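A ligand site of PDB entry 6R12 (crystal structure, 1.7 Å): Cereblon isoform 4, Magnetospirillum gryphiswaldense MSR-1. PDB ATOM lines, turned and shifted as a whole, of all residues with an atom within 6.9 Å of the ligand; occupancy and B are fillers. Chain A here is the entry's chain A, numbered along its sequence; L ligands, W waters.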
ATOM      1  N   VAL A  49      27.188   9.791 -17.603  1.00  0.00           N
ATOM      2  CA  VAL A  49      26.222   8.760 -17.787  1.00  0.00           C
ATOM      3  C   VAL A  49      26.808   7.372 -17.794  1.00  0.00           C
ATOM      4  O   VAL A  49      27.950   7.254 -17.802  1.00  0.00           O
ATOM      5  CB  VAL A  49      25.603   8.982 -19.188  1.00  0.00           C
ATOM      6  CG1 VAL A  49      24.951  10.353 -19.274  1.00  0.00           C
ATOM      7  CG2 VAL A  49      26.656   8.880 -20.268  1.00  0.00           C
ATOM      8  N   PHE A  50      25.974   6.337 -17.767  1.00  0.00           N
ATOM      9  CA  PHE A  50      26.461   4.990 -17.878  1.00  0.00           C
ATOM     10  C   PHE A  50      25.640   4.076 -18.766  1.00  0.00           C
ATOM     11  O   PHE A  50      24.465   4.239 -18.870  1.00  0.00           O
ATOM     12  CB  PHE A  50      26.716   4.384 -16.515  1.00  0.00           C
ATOM     13  CG  PHE A  50      25.499   3.990 -15.797  1.00  0.00           C
ATOM     14  CD1 PHE A  50      24.913   2.764 -16.017  1.00  0.00           C
ATOM     15  CD2 PHE A  50      24.949   4.819 -14.871  1.00  0.00           C
ATOM     16  CE1 PHE A  50      23.784   2.355 -15.314  1.00  0.00           C
ATOM     17  CE2 PHE A  50      23.813   4.421 -14.166  1.00  0.00           C
ATOM     18  CZ  PHE A  50      23.240   3.193 -14.381  1.00  0.00           C
ATOM     19  N   ASN A  51      26.285   3.135 -19.410  1.00  0.00           N
ATOM     20  CA  ASN A  51      25.604   2.219 -20.283  1.00  0.00           C
ATOM     21  C   ASN A  51      25.114   0.902 -19.600  1.00  0.00           C
ATOM     22  O   ASN A  51      25.345   0.703 -18.456  1.00  0.00           O
ATOM     23  CB  ASN A  51      26.395   1.983 -21.558  1.00  0.00           C
ATOM     24  CG  ASN A  51      27.614   1.136 -21.345  1.00  0.00           C
ATOM     25  OD1 ASN A  51      27.768   0.588 -20.291  1.00  0.00           O
ATOM     26  ND2 ASN A  51      28.442   1.016 -22.330  1.00  0.00           N
ATOM     27  N   PRO A  52      24.418   0.054 -20.325  1.00  0.00           N
ATOM     28  CA  PRO A  52      23.924  -1.159 -19.686  1.00  0.00           C
ATOM     29  C   PRO A  52      25.028  -2.070 -19.183  1.00  0.00           C
ATOM     30  O   PRO A  52      24.738  -2.876 -18.321  1.00  0.00           O
ATOM     31  CB  PRO A  52      23.039  -1.877 -20.742  1.00  0.00           C
ATOM     32  CG  PRO A  52      22.531  -0.642 -21.579  1.00  0.00           C
ATOM     33  CD  PRO A  52      23.710   0.327 -21.614  1.00  0.00           C
ATOM     34  N   ALA A  53      26.219  -1.911 -19.696  1.00  0.00           N
ATOM     35  CA  ALA A  53      27.392  -2.665 -19.263  1.00  0.00           C
ATOM     36  C   ALA A  53      28.103  -1.971 -18.105  1.00  0.00           C
ATOM     37  O   ALA A  53      29.217  -2.362 -17.762  1.00  0.00           O
ATOM     38  CB  ALA A  53      28.347  -2.926 -20.378  1.00  0.00           C
ATOM     39  N   MET A  55      29.575   0.873 -17.796  1.00  0.00           N
ATOM     40  CA  MET A  55      30.672   1.766 -18.110  1.00  0.00           C
ATOM     41  C   MET A  55      30.167   3.208 -17.992  1.00  0.00           C
ATOM     42  O   MET A  55      29.108   3.537 -18.524  1.00  0.00           O
ATOM     43  CB  MET A  55      31.161   1.521 -19.500  1.00  0.00           C
ATOM     44  CG  MET A  55      32.217   2.462 -20.003  1.00  0.00           C
ATOM     45  SD  MET A  55      33.623   2.540 -18.866  1.00  0.00           S
ATOM     46  CE  MET A  55      34.218   0.792 -18.970  1.00  0.00           C
ATOM     47  N   PHE A  57      30.699   7.244 -18.649  1.00  0.00           N
ATOM     48  CA  PHE A  57      31.283   8.122 -19.646  1.00  0.00           C
ATOM     49  C   PHE A  57      31.011   9.572 -19.273  1.00  0.00           C
ATOM     50  O   PHE A  57      29.979   9.960 -18.858  1.00  0.00           O
ATOM     51  CB  PHE A  57      30.687   7.915 -21.011  1.00  0.00           C
ATOM     52  CG  PHE A  57      30.804   6.473 -21.555  1.00  0.00           C
ATOM     53  CD1 PHE A  57      31.917   6.008 -22.214  1.00  0.00           C
ATOM     54  CD2 PHE A  57      29.741   5.578 -21.412  1.00  0.00           C
ATOM     55  CE1 PHE A  57      31.923   4.760 -22.804  1.00  0.00           C
ATOM     56  CE2 PHE A  57      29.822   4.326 -21.941  1.00  0.00           C
ATOM     57  CZ  PHE A  57      30.877   3.919 -22.643  1.00  0.00           C
ATOM     58  N   SER A  75      19.146   3.795 -32.914  1.00  0.00           N
ATOM     59  CA  SER A  75      18.345   3.061 -31.911  1.00  0.00           C
ATOM     60  C   SER A  75      17.930   4.102 -30.827  1.00  0.00           C
ATOM     61  O   SER A  75      18.773   4.905 -30.459  1.00  0.00           O
ATOM     62  CB  SER A  75      19.197   1.992 -31.219  1.00  0.00           C
ATOM     63  OG  SER A  75      18.346   1.347 -30.226  1.00  0.00           O
ATOM     64  N   GLY A  76      16.750   4.047 -30.317  1.00  0.00           N
ATOM     65  CA  GLY A  76      16.331   4.798 -29.146  1.00  0.00           C
ATOM     66  C   GLY A  76      16.553   4.108 -27.775  1.00  0.00           C
ATOM     67  O   GLY A  76      16.435   4.728 -26.765  1.00  0.00           O
ATOM     68  N   GLU A  77      16.956   2.839 -27.813  1.00  0.00           N
ATOM     69  CA  GLU A  77      17.067   2.043 -26.575  1.00  0.00           C
ATOM     70  C   GLU A  77      18.188   2.644 -25.683  1.00  0.00           C
ATOM     71  O   GLU A  77      19.261   2.924 -26.099  1.00  0.00           O
ATOM     72  CB  GLU A  77      17.456   0.595 -26.893  1.00  0.00           C
ATOM     73  CG  GLU A  77      16.508  -0.186 -27.732  1.00  0.00           C
ATOM     74  CD  GLU A  77      16.824  -1.712 -27.617  1.00  0.00           C
ATOM     75  OE1 GLU A  77      16.033  -2.478 -27.029  1.00  0.00           O
ATOM     76  OE2 GLU A  77      17.934  -2.112 -28.001  1.00  0.00           O
ATOM     77  N   PHE A  78      17.794   2.881 -24.444  1.00  0.00           N
ATOM     78  CA  PHE A  78      18.677   3.377 -23.380  1.00  0.00           C
ATOM     79  C   PHE A  78      19.203   4.746 -23.659  1.00  0.00           C
ATOM     80  O   PHE A  78      20.164   5.141 -23.057  1.00  0.00           O
ATOM     81  CB  PHE A  78      19.862   2.450 -23.150  1.00  0.00           C
ATOM     82  CG  PHE A  78      19.502   1.021 -22.932  1.00  0.00           C
ATOM     83  CD1 PHE A  78      18.766   0.650 -21.899  1.00  0.00           C
ATOM     84  CD2 PHE A  78      19.893   0.062 -23.879  1.00  0.00           C
ATOM     85  CE1 PHE A  78      18.462  -0.688 -21.627  1.00  0.00           C
ATOM     86  CE2 PHE A  78      19.560  -1.275 -23.689  1.00  0.00           C
ATOM     87  CZ  PHE A  78      18.908  -1.657 -22.541  1.00  0.00           C
ATOM     88  N   SER A  79      18.657   5.541 -24.602  1.00  0.00           N
ATOM     89  CA  SER A  79      19.168   6.794 -24.872  1.00  0.00           C
ATOM     90  C   SER A  79      19.273   7.683 -23.631  1.00  0.00           C
ATOM     91  O   SER A  79      18.278   7.833 -22.956  1.00  0.00           O
ATOM     92  CB  SER A  79      18.321   7.557 -25.928  1.00  0.00           C
ATOM     93  OG  SER A  79      18.939   8.784 -26.187  1.00  0.00           O
ATOM     94  N   TRP A  80      20.414   8.326 -23.528  1.00  0.00           N
ATOM     95  CA  TRP A  80      20.684   9.284 -22.468  1.00  0.00           C
ATOM     96  C   TRP A  80      20.018  10.620 -22.693  1.00  0.00           C
ATOM     97  O   TRP A  80      19.994  11.411 -21.755  1.00  0.00           O
ATOM     98  CB  TRP A  80      22.159   9.484 -22.268  1.00  0.00           C
ATOM     99  CG  TRP A  80      22.883   8.217 -21.827  1.00  0.00           C
ATOM    100  CD1 TRP A  80      22.520   7.414 -20.853  1.00  0.00           C
ATOM    101  CD2 TRP A  80      24.094   7.713 -22.397  1.00  0.00           C
ATOM    102  NE1 TRP A  80      23.475   6.344 -20.766  1.00  0.00           N
ATOM    103  CE2 TRP A  80      24.450   6.571 -21.664  1.00  0.00           C
ATOM    104  CE3 TRP A  80      24.908   8.112 -23.402  1.00  0.00           C
ATOM    105  CZ2 TRP A  80      25.553   5.845 -21.951  1.00  0.00           C
ATOM    106  CZ3 TRP A  80      25.988   7.336 -23.749  1.00  0.00           C
ATOM    107  CH2 TRP A  80      26.330   6.242 -23.001  1.00  0.00           C
ATOM    108  N   PHE A  81      19.471  10.867 -23.871  1.00  0.00           N
ATOM    109  CA  PHE A  81      18.938  12.217 -24.215  1.00  0.00           C
ATOM    110  C   PHE A  81      17.574  11.980 -24.738  1.00  0.00           C
ATOM    111  O   PHE A  81      17.392  11.297 -25.791  1.00  0.00           O
ATOM    112  CB  PHE A  81      19.869  12.945 -25.202  1.00  0.00           C
ATOM    113  CG  PHE A  81      21.260  13.129 -24.711  1.00  0.00           C
ATOM    114  CD1 PHE A  81      21.544  14.220 -23.866  1.00  0.00           C
ATOM    115  CD2 PHE A  81      22.231  12.270 -24.974  1.00  0.00           C
ATOM    116  CE1 PHE A  81      22.797  14.475 -23.447  1.00  0.00           C
ATOM    117  CE2 PHE A  81      23.533  12.505 -24.529  1.00  0.00           C
ATOM    118  CZ  PHE A  81      23.820  13.625 -23.739  1.00  0.00           C
ATOM    119  N   TYR A  84      15.970  11.397 -28.560  1.00  0.00           N
ATOM    120  CA  TYR A  84      16.980  11.178 -29.540  1.00  0.00           C
ATOM    121  C   TYR A  84      17.316   9.732 -29.641  1.00  0.00           C
ATOM    122  O   TYR A  84      17.318   9.000 -28.610  1.00  0.00           O
ATOM    123  CB  TYR A  84      18.237  11.918 -29.162  1.00  0.00           C
ATOM    124  CG  TYR A  84      18.147  13.381 -29.174  1.00  0.00           C
ATOM    125  CD1 TYR A  84      18.401  14.114 -30.292  1.00  0.00           C
ATOM    126  CD2 TYR A  84      17.832  14.067 -28.005  1.00  0.00           C
ATOM    127  CE1 TYR A  84      18.249  15.524 -30.287  1.00  0.00           C
ATOM    128  CE2 TYR A  84      17.737  15.484 -27.964  1.00  0.00           C
ATOM    129  CZ  TYR A  84      17.961  16.180 -29.141  1.00  0.00           C
ATOM    130  OH  TYR A  84      17.850  17.526 -29.070  1.00  0.00           O
ATOM    131  N   TRP A  86      20.314   7.063 -31.240  1.00  0.00           N
ATOM    132  CA  TRP A  86      21.751   7.127 -31.318  1.00  0.00           C
ATOM    133  C   TRP A  86      22.317   6.138 -32.295  1.00  0.00           C
ATOM    134  O   TRP A  86      21.746   5.013 -32.491  1.00  0.00           O
ATOM    135  CB  TRP A  86      22.438   6.878 -29.966  1.00  0.00           C
ATOM    136  CG  TRP A  86      22.004   5.713 -29.243  1.00  0.00           C
ATOM    137  CD1 TRP A  86      21.043   5.632 -28.300  1.00  0.00           C
ATOM    138  CD2 TRP A  86      22.521   4.348 -29.382  1.00  0.00           C
ATOM    139  NE1 TRP A  86      20.843   4.348 -27.936  1.00  0.00           N
ATOM    140  CE2 TRP A  86      21.743   3.526 -28.573  1.00  0.00           C
ATOM    141  CE3 TRP A  86      23.511   3.753 -30.212  1.00  0.00           C
ATOM    142  CZ2 TRP A  86      21.931   2.185 -28.502  1.00  0.00           C
ATOM    143  CZ3 TRP A  86      23.709   2.399 -30.094  1.00  0.00           C
ATOM    144  CH2 TRP A  86      22.945   1.637 -29.258  1.00  0.00           C
ATOM    145  N   THR A  87      23.493   6.522 -32.871  1.00  0.00           N
ATOM    146  CA  THR A  87      24.355   5.629 -33.620  1.00  0.00           C
ATOM    147  C   THR A  87      25.760   5.716 -33.050  1.00  0.00           C
ATOM    148  O   THR A  87      26.196   6.779 -32.670  1.00  0.00           O
ATOM    149  CB  THR A  87      24.313   6.126 -35.085  1.00  0.00           C
ATOM    150  OG1 THR A  87      22.921   6.273 -35.448  1.00  0.00           O
ATOM    151  CG2 THR A  87      24.876   5.223 -35.936  1.00  0.00           C
ATOM    152  N   ILE A  88      26.469   4.587 -33.007  1.00  0.00           N
ATOM    153  CA  ILE A  88      27.841   4.595 -32.543  1.00  0.00           C
ATOM    154  C   ILE A  88      28.702   5.389 -33.518  1.00  0.00           C
ATOM    155  O   ILE A  88      28.519   5.279 -34.780  1.00  0.00           O
ATOM    156  CB  ILE A  88      28.328   3.144 -32.501  1.00  0.00           C
ATOM    157  CG1 ILE A  88      27.651   2.512 -31.236  1.00  0.00           C
ATOM    158  CG2 ILE A  88      29.882   3.076 -32.303  1.00  0.00           C
ATOM    159  CD1 ILE A  88      27.878   1.034 -31.188  1.00  0.00           C
ATOM    160  N   HIS A  97      36.368   4.018 -30.541  1.00  0.00           N
ATOM    161  CA  HIS A  97      35.013   4.435 -30.249  1.00  0.00           C
ATOM    162  C   HIS A  97      35.027   5.786 -29.548  1.00  0.00           C
ATOM    163  O   HIS A  97      35.445   5.869 -28.411  1.00  0.00           O
ATOM    164  CB  HIS A  97      34.270   3.364 -29.440  1.00  0.00           C
ATOM    165  CG  HIS A  97      32.909   3.806 -29.043  1.00  0.00           C
ATOM    166  ND1 HIS A  97      32.278   3.322 -27.896  1.00  0.00           N
ATOM    167  CD2 HIS A  97      32.048   4.657 -29.647  1.00  0.00           C
ATOM    168  CE1 HIS A  97      31.078   3.881 -27.846  1.00  0.00           C
ATOM    169  NE2 HIS A  97      30.929   4.716 -28.850  1.00  0.00           N
ATOM    170  N   TRP A 100      28.852   8.966 -29.850  1.00  0.00           N
ATOM    171  CA  TRP A 100      27.571   8.623 -30.514  1.00  0.00           C
ATOM    172  C   TRP A 100      27.069   9.860 -31.265  1.00  0.00           C
ATOM    173  O   TRP A 100      27.325  10.987 -30.829  1.00  0.00           O
ATOM    174  CB  TRP A 100      26.487   8.146 -29.560  1.00  0.00           C
ATOM    175  CG  TRP A 100      26.917   6.973 -28.675  1.00  0.00           C
ATOM    176  CD1 TRP A 100      26.697   5.683 -28.935  1.00  0.00           C
ATOM    177  CD2 TRP A 100      27.743   7.008 -27.502  1.00  0.00           C
ATOM    178  NE1 TRP A 100      27.319   4.880 -27.953  1.00  0.00           N
ATOM    179  CE2 TRP A 100      27.937   5.703 -27.075  1.00  0.00           C
ATOM    180  CE3 TRP A 100      28.314   8.047 -26.727  1.00  0.00           C
ATOM    181  CZ2 TRP A 100      28.640   5.402 -25.904  1.00  0.00           C
ATOM    182  CZ3 TRP A 100      29.058   7.693 -25.547  1.00  0.00           C
ATOM    183  CH2 TRP A 100      29.260   6.422 -25.225  1.00  0.00           C
ATOM    184  N   TYR A 102      23.538  11.559 -32.317  1.00  0.00           N
ATOM    185  CA  TYR A 102      22.156  11.567 -31.892  1.00  0.00           C
ATOM    186  C   TYR A 102      21.301  12.284 -32.945  1.00  0.00           C
ATOM    187  O   TYR A 102      21.755  13.270 -33.499  1.00  0.00           O
ATOM    188  CB  TYR A 102      22.029  12.310 -30.549  1.00  0.00           C
ATOM    189  CG  TYR A 102      22.593  11.472 -29.390  1.00  0.00           C
ATOM    190  CD1 TYR A 102      21.802  10.515 -28.826  1.00  0.00           C
ATOM    191  CD2 TYR A 102      23.928  11.658 -29.013  1.00  0.00           C
ATOM    192  CE1 TYR A 102      22.255   9.751 -27.685  1.00  0.00           C
ATOM    193  CE2 TYR A 102      24.447  10.906 -27.959  1.00  0.00           C
ATOM    194  CZ  TYR A 102      23.618   9.964 -27.330  1.00  0.00           C
ATOM    195  OH  TYR A 102      24.201   9.242 -26.289  1.00  0.00           O
HETATM  196  O1  LIG L   1      23.468   3.293 -23.071  1.00  0.00           O
HETATM  197  C1  LIG L   1      23.677   4.004 -24.042  1.00  0.00           C
HETATM  198  N1  LIG L   1      22.980   5.174 -24.218  1.00  0.00           N
HETATM  199  C2  LIG L   1      23.124   6.075 -25.256  1.00  0.00           C
HETATM  200  O2  LIG L   1      22.534   7.141 -25.238  1.00  0.00           O
HETATM  201  C3  LIG L   1      24.034   5.686 -26.387  1.00  0.00           C
HETATM  202  C4  LIG L   1      24.280   4.197 -26.474  1.00  0.00           C
HETATM  203  C5  LIG L   1      24.710   3.669 -25.112  1.00  0.00           C
HETATM  204  N2  LIG L   1      24.953   2.240 -25.104  1.00  0.00           N
HETATM  205  C6  LIG L   1      26.367  -2.147 -24.788  1.00  0.00           C
HETATM  206  C7  LIG L   1      26.878  -0.853 -24.742  1.00  0.00           C
HETATM  207  C8  LIG L   1      25.981   0.184 -24.914  1.00  0.00           C
HETATM  208  C9  LIG L   1      24.638  -0.047 -25.129  1.00  0.00           C
HETATM  209  O3  LIG L   1      27.252   2.268 -24.808  1.00  0.00           O
HETATM  210  O4  LIG L   1      22.788   1.503 -25.494  1.00  0.00           O
HETATM  211  C10 LIG L   1      24.126  -1.320 -25.165  1.00  0.00           C
HETATM  212  C11 LIG L   1      25.013  -2.378 -24.994  1.00  0.00           C
HETATM  213  C12 LIG L   1      23.954   1.270 -25.275  1.00  0.00           C
HETATM  214  C13 LIG L   1      26.207   1.655 -24.927  1.00  0.00           C
HETATM  215  O   HOH W   1      26.955   2.125 -27.814  1.00  0.00           O
HETATM  216  O   HOH W   2      21.351  -0.757 -26.973  1.00  0.00           O
HETATM  217  O   HOH W   3      29.515   2.041 -25.798  1.00  0.00           O
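OH of Tyr 102 is in hydrogen-bond range of O2 of the ligand, 2.9 Å away. N of Trp 80 sits at hydrogen-bond distance from O2 of the ligand (3.0 Å). The backbone carbonyl oxygen (O) of Phe 78 lies within hydrogen-bond range of a nitrogen (N1) of the ligand, 3.0 Å away. ND2 of Asn 51 lies within hydrogen-bond range of O3 of the ligand (3.0 Å).
The indole nitrogen (NE1) of Trp 86 sits at hydrogen-bond distance from the backbone carbonyl oxygen (O) of Glu 77 (2.8 Å). OD1 of Asn 51 lies within hydrogen-bond range of N of Met 55 (3.1 Å). The backbone carbonyl oxygen of Phe 50 sits at hydrogen-bond distance from the indole nitrogen of Trp 80. OG of Ser 75 sits at hydrogen-bond distance from N of Glu 77. N of Trp 86 lies within hydrogen-bond range of O of Ser 75 (2.8 Å). The backbone carbonyl oxygen of Tyr 84 sits at hydrogen-bond distance from the side-chain hydroxyl of Ser 79 (2.9 Å). The side-chain hydroxyl (OG) of Ser 79 is in hydrogen-bond range of the backbone carbonyl oxygen (O) of Phe 81. The side-chain amide oxygen (OD1) of Asn 51 lies within hydrogen-bond range of the backbone NH (N) of Ala 53, at 3.0 Å.
Pro 52 touches the ligand. Glu 77 touches the ligand. Ser 79 touches the ligand. Trp 86 touches the ligand (CZ2 to O4, 3.2 Å). Trp 100 touches the ligand (NE1 to C4, 3.4 Å). The nearest printed residue that does not touch the ligand is Phe 57 (4.4 Å).
Water W1 bridges NE1 of Trp 100 and O3 of the ligand.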
